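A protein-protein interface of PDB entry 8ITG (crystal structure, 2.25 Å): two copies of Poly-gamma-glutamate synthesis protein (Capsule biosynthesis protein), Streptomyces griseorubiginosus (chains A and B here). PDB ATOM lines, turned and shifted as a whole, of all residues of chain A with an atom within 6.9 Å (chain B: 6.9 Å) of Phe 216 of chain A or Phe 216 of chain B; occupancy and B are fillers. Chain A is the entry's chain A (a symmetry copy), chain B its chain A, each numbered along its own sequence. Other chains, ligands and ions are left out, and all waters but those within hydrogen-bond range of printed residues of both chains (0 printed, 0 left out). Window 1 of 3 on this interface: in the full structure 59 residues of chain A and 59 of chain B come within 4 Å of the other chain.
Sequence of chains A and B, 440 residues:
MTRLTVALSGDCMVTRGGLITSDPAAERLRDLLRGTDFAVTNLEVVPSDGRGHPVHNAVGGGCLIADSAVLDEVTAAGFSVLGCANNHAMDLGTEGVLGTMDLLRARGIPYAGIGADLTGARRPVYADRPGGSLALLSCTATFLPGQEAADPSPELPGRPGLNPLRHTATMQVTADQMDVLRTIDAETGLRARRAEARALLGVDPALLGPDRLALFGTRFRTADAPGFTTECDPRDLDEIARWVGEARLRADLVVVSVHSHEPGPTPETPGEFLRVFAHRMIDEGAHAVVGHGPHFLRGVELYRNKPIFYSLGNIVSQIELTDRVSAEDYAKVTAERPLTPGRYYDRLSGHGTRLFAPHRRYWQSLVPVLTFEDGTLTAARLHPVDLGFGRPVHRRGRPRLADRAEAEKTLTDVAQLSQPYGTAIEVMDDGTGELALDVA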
ATOM      1  N   MET A 171      10.782  12.589  14.780  1.00  0.00           N
ATOM      2  CA  MET A 171       9.724  12.270  15.728  1.00  0.00           C
ATOM      3  C   MET A 171       9.592  10.754  15.822  1.00  0.00           C
ATOM      4  O   MET A 171       9.284  10.093  14.824  1.00  0.00           O
ATOM      5  CB  MET A 171       8.404  12.899  15.288  1.00  0.00           C
ATOM      6  CG  MET A 171       8.496  14.387  15.000  1.00  0.00           C
ATOM      7  SD  MET A 171       8.265  15.382  16.480  1.00  0.00           S
ATOM      8  CE  MET A 171       6.531  15.077  16.807  1.00  0.00           C
ATOM      9  N   LEU A 181      -0.992   8.645  10.927  1.00  0.00           N
ATOM     10  CA  LEU A 181      -0.366   9.666  10.091  1.00  0.00           C
ATOM     11  C   LEU A 181      -0.458   9.302   8.613  1.00  0.00           C
ATOM     12  O   LEU A 181      -0.783  10.149   7.772  1.00  0.00           O
ATOM     13  CB  LEU A 181       1.091   9.863  10.511  1.00  0.00           C
ATOM     14  CG  LEU A 181       1.296  10.457  11.903  1.00  0.00           C
ATOM     15  CD1 LEU A 181       2.766  10.458  12.278  1.00  0.00           C
ATOM     16  CD2 LEU A 181       0.728  11.863  11.964  1.00  0.00           C
ATOM     17  N   ARG A 182      -0.171   8.041   8.275  1.00  0.00           N
ATOM     18  CA  ARG A 182      -0.334   7.598   6.895  1.00  0.00           C
ATOM     19  C   ARG A 182      -1.791   7.679   6.461  1.00  0.00           C
ATOM     20  O   ARG A 182      -2.088   8.035   5.314  1.00  0.00           O
ATOM     21  CB  ARG A 182       0.182   6.169   6.729  1.00  0.00           C
ATOM     22  CG  ARG A 182       1.658   5.980   7.022  1.00  0.00           C
ATOM     23  CD  ARG A 182       2.253   4.949   6.075  1.00  0.00           C
ATOM     24  NE  ARG A 182       3.305   4.158   6.702  1.00  0.00           N
ATOM     25  CZ  ARG A 182       3.155   2.902   7.106  1.00  0.00           C
ATOM     26  NH1 ARG A 182       4.168   2.259   7.670  1.00  0.00           N
ATOM     27  NH2 ARG A 182       1.992   2.285   6.940  1.00  0.00           N
ATOM     28  N   ILE A 184      -4.099   9.803   7.603  1.00  0.00           N
ATOM     29  CA  ILE A 184      -4.366  11.217   7.354  1.00  0.00           C
ATOM     30  C   ILE A 184      -3.785  11.636   6.011  1.00  0.00           C
ATOM     31  O   ILE A 184      -4.410  12.384   5.251  1.00  0.00           O
ATOM     32  CB  ILE A 184      -3.807  12.076   8.503  1.00  0.00           C
ATOM     33  CG1 ILE A 184      -4.529  11.756   9.812  1.00  0.00           C
ATOM     34  CG2 ILE A 184      -3.927  13.558   8.180  1.00  0.00           C
ATOM     35  CD1 ILE A 184      -3.939  12.456  11.013  1.00  0.00           C
ATOM     36  N   ASP A 185      -2.584  11.147   5.693  1.00  0.00           N
ATOM     37  CA  ASP A 185      -1.955  11.479   4.419  1.00  0.00           C
ATOM     38  C   ASP A 185      -2.812  11.021   3.245  1.00  0.00           C
ATOM     39  O   ASP A 185      -3.009  11.763   2.276  1.00  0.00           O
ATOM     40  CB  ASP A 185      -0.560  10.854   4.357  1.00  0.00           C
ATOM     41  CG  ASP A 185       0.111  11.050   3.012  1.00  0.00           C
ATOM     42  OD1 ASP A 185       0.324  12.214   2.613  1.00  0.00           O
ATOM     43  OD2 ASP A 185       0.434  10.036   2.361  1.00  0.00           O
ATOM     44  N   THR A 188      -6.817  12.753   3.437  1.00  0.00           N
ATOM     45  CA  THR A 188      -6.961  14.174   3.139  1.00  0.00           C
ATOM     46  C   THR A 188      -6.766  14.476   1.659  1.00  0.00           C
ATOM     47  O   THR A 188      -7.135  15.564   1.207  1.00  0.00           O
ATOM     48  CB  THR A 188      -5.964  15.002   3.950  1.00  0.00           C
ATOM     49  OG1 THR A 188      -4.634  14.543   3.684  1.00  0.00           O
ATOM     50  CG2 THR A 188      -6.263  14.900   5.442  1.00  0.00           C
ATOM     51  N   LEU A 190      -3.631  14.388   0.522  1.00  0.00           N
ATOM     52  CA  LEU A 190      -2.246  14.844   0.465  1.00  0.00           C
ATOM     53  C   LEU A 190      -1.390  13.901  -0.371  1.00  0.00           C
ATOM     54  O   LEU A 190      -0.548  14.350  -1.156  1.00  0.00           O
ATOM     55  CB  LEU A 190      -1.681  14.970   1.880  1.00  0.00           C
ATOM     56  CG  LEU A 190      -0.271  15.548   1.997  1.00  0.00           C
ATOM     57  CD1 LEU A 190      -0.253  16.988   1.512  1.00  0.00           C
ATOM     58  CD2 LEU A 190       0.235  15.449   3.428  1.00  0.00           C
ATOM     59  N   ARG A 194       0.978  14.124  -4.538  1.00  0.00           N
ATOM     60  CA  ARG A 194       2.338  13.718  -4.856  1.00  0.00           C
ATOM     61  C   ARG A 194       2.389  12.732  -6.015  1.00  0.00           C
ATOM     62  O   ARG A 194       3.445  12.143  -6.268  1.00  0.00           O
ATOM     63  CB  ARG A 194       3.017  13.111  -3.627  1.00  0.00           C
ATOM     64  CG  ARG A 194       3.078  14.039  -2.425  1.00  0.00           C
ATOM     65  CD  ARG A 194       4.030  13.504  -1.367  1.00  0.00           C
ATOM     66  NE  ARG A 194       3.690  12.145  -0.958  1.00  0.00           N
ATOM     67  CZ  ARG A 194       2.880  11.848   0.052  1.00  0.00           C
ATOM     68  NH1 ARG A 194       2.320  12.819   0.761  1.00  0.00           N
ATOM     69  NH2 ARG A 194       2.628  10.582   0.353  1.00  0.00           N
ATOM     70  N   ALA A 214       8.276  10.668   5.820  1.00  0.00           N
ATOM     71  CA  ALA A 214       8.449  12.112   5.670  1.00  0.00           C
ATOM     72  C   ALA A 214       7.101  12.701   5.289  1.00  0.00           C
ATOM     73  O   ALA A 214       6.671  12.577   4.139  1.00  0.00           O
ATOM     74  CB  ALA A 214       9.503  12.455   4.615  1.00  0.00           C
ATOM     75  N   LEU A 215       6.432  13.319   6.256  1.00  0.00           N
ATOM     76  CA  LEU A 215       5.143  13.956   6.038  1.00  0.00           C
ATOM     77  C   LEU A 215       5.168  15.347   6.647  1.00  0.00           C
ATOM     78  O   LEU A 215       5.816  15.576   7.671  1.00  0.00           O
ATOM     79  CB  LEU A 215       3.998  13.155   6.664  1.00  0.00           C
ATOM     80  CG  LEU A 215       3.789  11.734   6.143  1.00  0.00           C
ATOM     81  CD1 LEU A 215       2.972  10.910   7.125  1.00  0.00           C
ATOM     82  CD2 LEU A 215       3.124  11.748   4.774  1.00  0.00           C
ATOM     83  N   PHE A 216       4.455  16.273   6.002  1.00  0.00           N
ATOM     84  CA  PHE A 216       4.311  17.646   6.494  1.00  0.00           C
ATOM     85  C   PHE A 216       5.668  18.311   6.704  1.00  0.00           C
ATOM     86  O   PHE A 216       5.832  19.164   7.580  1.00  0.00           O
ATOM     87  CB  PHE A 216       3.486  17.690   7.783  1.00  0.00           C
ATOM     88  CG  PHE A 216       2.390  16.657   7.843  1.00  0.00           C
ATOM     89  CD1 PHE A 216       1.308  16.724   6.981  1.00  0.00           C
ATOM     90  CD2 PHE A 216       2.438  15.628   8.769  1.00  0.00           C
ATOM     91  CE1 PHE A 216       0.301  15.777   7.035  1.00  0.00           C
ATOM     92  CE2 PHE A 216       1.434  14.678   8.830  1.00  0.00           C
ATOM     93  CZ  PHE A 216       0.363  14.754   7.960  1.00  0.00           C
ATOM     94  N   GLY A 217       6.652  17.921   5.898  1.00  0.00           N
ATOM     95  CA  GLY A 217       8.006  18.423   6.079  1.00  0.00           C
ATOM     96  C   GLY A 217       8.636  18.026   7.393  1.00  0.00           C
ATOM     97  O   GLY A 217       9.425  18.797   7.951  1.00  0.00           O
ATOM     98  N   THR A 218       8.308  16.843   7.910  1.00  0.00           N
ATOM     99  CA  THR A 218       8.840  16.374   9.181  1.00  0.00           C
ATOM    100  C   THR A 218       9.160  14.890   9.070  1.00  0.00           C
ATOM    101  O   THR A 218       8.512  14.158   8.319  1.00  0.00           O
ATOM    102  CB  THR A 218       7.852  16.621  10.332  1.00  0.00           C
ATOM    103  OG1 THR A 218       7.247  17.908  10.168  1.00  0.00           O
ATOM    104  CG2 THR A 218       8.563  16.576  11.678  1.00  0.00           C
ATOM    105  N   ARG A 219      10.164  14.455   9.825  1.00  0.00           N
ATOM    106  CA  ARG A 219      10.592  13.063   9.819  1.00  0.00           C
ATOM    107  C   ARG A 219       9.897  12.294  10.936  1.00  0.00           C
ATOM    108  O   ARG A 219       9.900  12.725  12.094  1.00  0.00           O
ATOM    109  CB  ARG A 219      12.111  12.970   9.973  1.00  0.00           C
ATOM    110  CG  ARG A 219      12.877  13.268   8.695  1.00  0.00           C
ATOM    111  CD  ARG A 219      14.280  13.781   8.987  1.00  0.00           C
ATOM    112  NE  ARG A 219      15.160  13.647   7.830  1.00  0.00           N
ATOM    113  CZ  ARG A 219      15.143  14.455   6.773  1.00  0.00           C
ATOM    114  NH1 ARG A 219      14.283  15.465   6.714  1.00  0.00           N
ATOM    115  NH2 ARG A 219      15.985  14.251   5.769  1.00  0.00           N
ATOM    116  N   PHE A 220       9.302  11.158  10.583  1.00  0.00           N
ATOM    117  CA  PHE A 220       8.647  10.278  11.537  1.00  0.00           C
ATOM    118  C   PHE A 220       9.265   8.889  11.452  1.00  0.00           C
ATOM    119  O   PHE A 220       9.539   8.389  10.356  1.00  0.00           O
ATOM    120  CB  PHE A 220       7.137  10.193  11.277  1.00  0.00           C
ATOM    121  CG  PHE A 220       6.402  11.478  11.540  1.00  0.00           C
ATOM    122  CD1 PHE A 220       6.025  11.823  12.825  1.00  0.00           C
ATOM    123  CD2 PHE A 220       6.076  12.331  10.498  1.00  0.00           C
ATOM    124  CE1 PHE A 220       5.345  13.001  13.071  1.00  0.00           C
ATOM    125  CE2 PHE A 220       5.393  13.512  10.737  1.00  0.00           C
ATOM    126  CZ  PHE A 220       5.027  13.847  12.024  1.00  0.00           C
ATOM    127  N   MET B 171      -5.140  21.128   6.178  1.00  0.00           N
ATOM    128  CA  MET B 171      -5.542  19.730   6.228  1.00  0.00           C
ATOM    129  C   MET B 171      -6.798  19.613   7.083  1.00  0.00           C
ATOM    130  O   MET B 171      -6.774  19.941   8.275  1.00  0.00           O
ATOM    131  CB  MET B 171      -4.418  18.870   6.803  1.00  0.00           C
ATOM    132  CG  MET B 171      -3.080  19.065   6.113  1.00  0.00           C
ATOM    133  SD  MET B 171      -2.899  18.010   4.667  1.00  0.00           S
ATOM    134  CE  MET B 171      -2.790  16.405   5.451  1.00  0.00           C
ATOM    135  N   LEU B 181      -3.035  13.700  16.640  1.00  0.00           N
ATOM    136  CA  LEU B 181      -1.978  14.658  16.325  1.00  0.00           C
ATOM    137  C   LEU B 181      -1.542  15.427  17.568  1.00  0.00           C
ATOM    138  O   LEU B 181      -0.343  15.608  17.812  1.00  0.00           O
ATOM    139  CB  LEU B 181      -2.451  15.618  15.234  1.00  0.00           C
ATOM    140  CG  LEU B 181      -2.690  14.985  13.864  1.00  0.00           C
ATOM    141  CD1 LEU B 181      -3.307  15.987  12.906  1.00  0.00           C
ATOM    142  CD2 LEU B 181      -1.389  14.440  13.302  1.00  0.00           C
ATOM    143  N   ARG B 182      -2.506  15.891  18.369  1.00  0.00           N
ATOM    144  CA  ARG B 182      -2.162  16.548  19.625  1.00  0.00           C
ATOM    145  C   ARG B 182      -1.452  15.588  20.569  1.00  0.00           C
ATOM    146  O   ARG B 182      -0.520  15.979  21.282  1.00  0.00           O
ATOM    147  CB  ARG B 182      -3.415  17.110  20.295  1.00  0.00           C
ATOM    148  CG  ARG B 182      -4.152  18.168  19.497  1.00  0.00           C
ATOM    149  CD  ARG B 182      -4.726  19.223  20.430  1.00  0.00           C
ATOM    150  NE  ARG B 182      -5.994  19.761  19.949  1.00  0.00           N
ATOM    151  CZ  ARG B 182      -7.179  19.446  20.458  1.00  0.00           C
ATOM    152  NH1 ARG B 182      -8.283  19.983  19.956  1.00  0.00           N
ATOM    153  NH2 ARG B 182      -7.262  18.599  21.476  1.00  0.00           N
ATOM    154  N   ILE B 184       0.442  12.977  19.710  1.00  0.00           N
ATOM    155  CA  ILE B 184       1.808  12.856  19.209  1.00  0.00           C
ATOM    156  C   ILE B 184       2.624  14.080  19.597  1.00  0.00           C
ATOM    157  O   ILE B 184       3.793  13.971  19.986  1.00  0.00           O
ATOM    158  CB  ILE B 184       1.799  12.643  17.683  1.00  0.00           C
ATOM    159  CG1 ILE B 184       1.122  11.319  17.330  1.00  0.00           C
ATOM    160  CG2 ILE B 184       3.212  12.684  17.122  1.00  0.00           C
ATOM    161  CD1 ILE B 184       0.949  11.107  15.845  1.00  0.00           C
ATOM    162  N   ASP B 185       2.015  15.265  19.510  1.00  0.00           N
ATOM    163  CA  ASP B 185       2.712  16.493  19.877  1.00  0.00           C
ATOM    164  C   ASP B 185       3.153  16.461  21.338  1.00  0.00           C
ATOM    165  O   ASP B 185       4.288  16.823  21.664  1.00  0.00           O
ATOM    166  CB  ASP B 185       1.810  17.697  19.604  1.00  0.00           C
ATOM    167  CG  ASP B 185       2.417  19.004  20.075  1.00  0.00           C
ATOM    168  OD1 ASP B 185       3.505  19.371  19.585  1.00  0.00           O
ATOM    169  OD2 ASP B 185       1.796  19.667  20.930  1.00  0.00           O
ATOM    170  N   THR B 188       5.685  12.997  22.151  1.00  0.00           N
ATOM    171  CA  THR B 188       7.043  13.005  21.619  1.00  0.00           C
ATOM    172  C   THR B 188       7.944  13.991  22.350  1.00  0.00           C
ATOM    173  O   THR B 188       9.169  13.910  22.217  1.00  0.00           O
ATOM    174  CB  THR B 188       7.040  13.345  20.129  1.00  0.00           C
ATOM    175  OG1 THR B 188       6.392  14.606  19.929  1.00  0.00           O
ATOM    176  CG2 THR B 188       6.330  12.260  19.326  1.00  0.00           C
ATOM    177  N   LEU B 190       7.482  17.222  21.662  1.00  0.00           N
ATOM    178  CA  LEU B 190       7.471  18.384  20.778  1.00  0.00           C
ATOM    179  C   LEU B 190       6.839  19.590  21.461  1.00  0.00           C
ATOM    180  O   LEU B 190       7.335  20.714  21.333  1.00  0.00           O
ATOM    181  CB  LEU B 190       6.729  18.049  19.485  1.00  0.00           C
ATOM    182  CG  LEU B 190       6.729  19.129  18.404  1.00  0.00           C
ATOM    183  CD1 LEU B 190       8.145  19.375  17.910  1.00  0.00           C
ATOM    184  CD2 LEU B 190       5.810  18.743  17.254  1.00  0.00           C
ATOM    185  N   ARG B 194       8.315  23.887  23.002  1.00  0.00           N
ATOM    186  CA  ARG B 194       7.727  25.201  22.793  1.00  0.00           C
ATOM    187  C   ARG B 194       7.454  25.926  24.103  1.00  0.00           C
ATOM    188  O   ARG B 194       6.774  26.957  24.100  1.00  0.00           O
ATOM    189  CB  ARG B 194       6.434  25.086  21.982  1.00  0.00           C
ATOM    190  CG  ARG B 194       6.605  24.431  20.622  1.00  0.00           C
ATOM    191  CD  ARG B 194       5.372  24.636  19.756  1.00  0.00           C
ATOM    192  NE  ARG B 194       4.156  24.165  20.411  1.00  0.00           N
ATOM    193  CZ  ARG B 194       3.668  22.935  20.287  1.00  0.00           C
ATOM    194  NH1 ARG B 194       4.297  22.045  19.532  1.00  0.00           N
ATOM    195  NH2 ARG B 194       2.554  22.595  20.920  1.00  0.00           N
ATOM    196  N   ALA B 214      -1.681  24.169  14.487  1.00  0.00           N
ATOM    197  CA  ALA B 214      -0.469  24.355  13.691  1.00  0.00           C
ATOM    198  C   ALA B 214       0.601  23.440  14.261  1.00  0.00           C
ATOM    199  O   ALA B 214       1.180  23.738  15.311  1.00  0.00           O
ATOM    200  CB  ALA B 214       0.005  25.809  13.702  1.00  0.00           C
ATOM    201  N   LEU B 215       0.848  22.325  13.584  1.00  0.00           N
ATOM    202  CA  LEU B 215       1.862  21.365  13.989  1.00  0.00           C
ATOM    203  C   LEU B 215       2.711  21.002  12.783  1.00  0.00           C
ATOM    204  O   LEU B 215       2.215  20.952  11.654  1.00  0.00           O
ATOM    205  CB  LEU B 215       1.243  20.090  14.569  1.00  0.00           C
ATOM    206  CG  LEU B 215       0.383  20.254  15.821  1.00  0.00           C
ATOM    207  CD1 LEU B 215      -0.524  19.049  16.017  1.00  0.00           C
ATOM    208  CD2 LEU B 215       1.248  20.476  17.052  1.00  0.00           C
ATOM    209  N   PHE B 216       3.998  20.749  13.036  1.00  0.00           N
ATOM    210  CA  PHE B 216       4.938  20.313  12.001  1.00  0.00           C
ATOM    211  C   PHE B 216       4.981  21.295  10.833  1.00  0.00           C
ATOM    212  O   PHE B 216       5.215  20.911   9.685  1.00  0.00           O
ATOM    213  CB  PHE B 216       4.601  18.903  11.504  1.00  0.00           C
ATOM    214  CG  PHE B 216       4.048  17.996  12.572  1.00  0.00           C
ATOM    215  CD1 PHE B 216       4.839  17.586  13.633  1.00  0.00           C
ATOM    216  CD2 PHE B 216       2.740  17.543  12.506  1.00  0.00           C
ATOM    217  CE1 PHE B 216       4.332  16.753  14.613  1.00  0.00           C
ATOM    218  CE2 PHE B 216       2.226  16.708  13.483  1.00  0.00           C
ATOM    219  CZ  PHE B 216       3.026  16.313  14.539  1.00  0.00           C
ATOM    220  N   GLY B 217       4.752  22.573  11.123  1.00  0.00           N
ATOM    221  CA  GLY B 217       4.676  23.573  10.071  1.00  0.00           C
ATOM    222  C   GLY B 217       3.530  23.364   9.107  1.00  0.00           C
ATOM    223  O   GLY B 217       3.663  23.678   7.920  1.00  0.00           O
ATOM    224  N   THR B 218       2.403  22.836   9.585  1.00  0.00           N
ATOM    225  CA  THR B 218       1.248  22.573   8.739  1.00  0.00           C
ATOM    226  C   THR B 218      -0.019  22.942   9.497  1.00  0.00           C
ATOM    227  O   THR B 218      -0.069  22.853  10.726  1.00  0.00           O
ATOM    228  CB  THR B 218       1.194  21.100   8.300  1.00  0.00           C
ATOM    229  OG1 THR B 218       2.516  20.656   7.975  1.00  0.00           O
ATOM    230  CG2 THR B 218       0.300  20.930   7.080  1.00  0.00           C
ATOM    231  N   ARG B 219      -1.040  23.358   8.754  1.00  0.00           N
ATOM    232  CA  ARG B 219      -2.313  23.755   9.337  1.00  0.00           C
ATOM    233  C   ARG B 219      -3.276  22.575   9.354  1.00  0.00           C
ATOM    234  O   ARG B 219      -3.476  21.912   8.331  1.00  0.00           O
ATOM    235  CB  ARG B 219      -2.917  24.925   8.558  1.00  0.00           C
ATOM    236  CG  ARG B 219      -2.287  26.269   8.882  1.00  0.00           C
ATOM    237  CD  ARG B 219      -2.422  27.248   7.723  1.00  0.00           C
ATOM    238  NE  ARG B 219      -2.240  28.630   8.155  1.00  0.00           N
ATOM    239  CZ  ARG B 219      -1.061  29.189   8.418  1.00  0.00           C
ATOM    240  NH1 ARG B 219       0.057  28.482   8.301  1.00  0.00           N
ATOM    241  NH2 ARG B 219      -0.999  30.455   8.805  1.00  0.00           N
ATOM    242  N   PHE B 220      -3.866  22.317  10.517  1.00  0.00           N
ATOM    243  CA  PHE B 220      -4.855  21.263  10.686  1.00  0.00           C
ATOM    244  C   PHE B 220      -6.145  21.863  11.230  1.00  0.00           C
ATOM    245  O   PHE B 220      -6.114  22.721  12.118  1.00  0.00           O
ATOM    246  CB  PHE B 220      -4.350  20.166  11.632  1.00  0.00           C
ATOM    247  CG  PHE B 220      -3.197  19.374  11.084  1.00  0.00           C
ATOM    248  CD1 PHE B 220      -3.415  18.328  10.205  1.00  0.00           C
ATOM    249  CD2 PHE B 220      -1.895  19.667  11.459  1.00  0.00           C
ATOM    250  CE1 PHE B 220      -2.358  17.593   9.703  1.00  0.00           C
ATOM    251  CE2 PHE B 220      -0.832  18.934  10.960  1.00  0.00           C
ATOM    252  CZ  PHE B 220      -1.063  17.896  10.082  1.00  0.00           C
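Of chain B, only Met 171, Phe 216, Thr 218 and Phe 220 come within 4 Å of Phe 216 of chain A. Phe 216 of chain B touches just these residues of chain A: Met 171 (3.5 Å), Phe 216 (2.8 Å), Thr 218 (3.1 Å) and Phe 220 (3.95 Å). Of the printed residues of chain B, Thr 188 of chain A touches Met 171. Printed residues of chain B within 4 Å of Leu 190 of chain A: Met 171. Arg 182 of chain A touches none of the printed residues of chain B. Arg 219 of chain A touches none of the printed residues of chain B. The nearest residue of chain B that does not touch Phe 216 of chain A is Gly 217 of chain B (5.0 Å).
The backbone carbonyl oxygen of Phe 216 of chain A sits close to the backbone carbonyl oxygen of Phe 216 of chain B, at 2.8 Å.
Of the 15 printed residues of chain B, 8 touch a printed residue of chain A. Hydrophobic or aromatic side chains of chain B within 4 Å of the printed part of chain A: Met 171, Leu 181, Ile 184, Leu 190, Phe 216 and Phe 220. Hydrophobic or aromatic side chains of chain A that line the printed part of chain B: Met 171, Leu 181, Ile 184, Leu 190, Phe 216 and Phe 220. Along chain A the printed residues that touch a printed residue of chain B span positions 171 to 220. Among the printed residues, no Asp or Glu carboxylate lies within 4 Å of a Lys or Arg side-chain nitrogen of the other chain.
The backbone carbonyl oxygen (O) of Asp 185 of chain A is in hydrogen-bond range of the backbone NH (N) of Leu 190 of chain A (3.2 Å). O of Asp 185 of chain B is in hydrogen-bond range of N of Leu 190 of chain B, at 3.2 Å. O of Ile 184 of chain A is in hydrogen-bond range of OG1 of Thr 188 of chain A. The backbone NH of Met 171 of chain A lies within hydrogen-bond range of the backbone carbonyl oxygen of Arg 219 of chain A, at 2.8 Å. O of Phe 216 of chain B sits at hydrogen-bond distance from OG1 of Thr 218 of chain B. The side-chain hydroxyl (OG1) of Thr 188 of chain B lies within hydrogen-bond range of the backbone NH (N) of Leu 190 of chain B, at 3.3 Å.
Met 171 of chain A touches Thr 188 of chain B, and with the chains exchanged Thr 188 of chain A touches Met 171 of chain B. Met 171 of chain A touches Phe 216 of chain B, and with the chains exchanged Phe 216 of chain A touches Met 171 of chain B. Leu 181 of chain A touches Ile 184 of chain B, and with the chains exchanged Ile 184 of chain A touches Leu 181 of chain B. Phe 216 of chain A touches Phe 220 of chain B, and with the chains exchanged Phe 220 of chain A touches Phe 216 of chain B.
Met 171 of chain A touches Thr 188 of chain B. Leu 190 of chain B touches Met 171 of chain A (CD2 to CE, 3.8 Å). Leu 181 of chain B touches Leu 181 of chain A (CD2 to CD2, 3.6 Å). CD1 of Ile 184 of chain B touches CD2 of Leu 181 of chain A (3.96 Å). Ile 184 of chain A touches Leu 181 of chain B. OG1 of Thr 188 of chain A touches CE of Met 171 of chain B, at 3.2 Å. Leu 190 of chain A touches Met 171 of chain B. Met 171 of chain B touches Phe 216 of chain A. CB of Phe 216 of chain A touches OG1 of Thr 218 of chain B, at 3.1 Å. Phe 220 of chain A touches Phe 216 of chain B (CZ to CE1, 3.95 Å).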
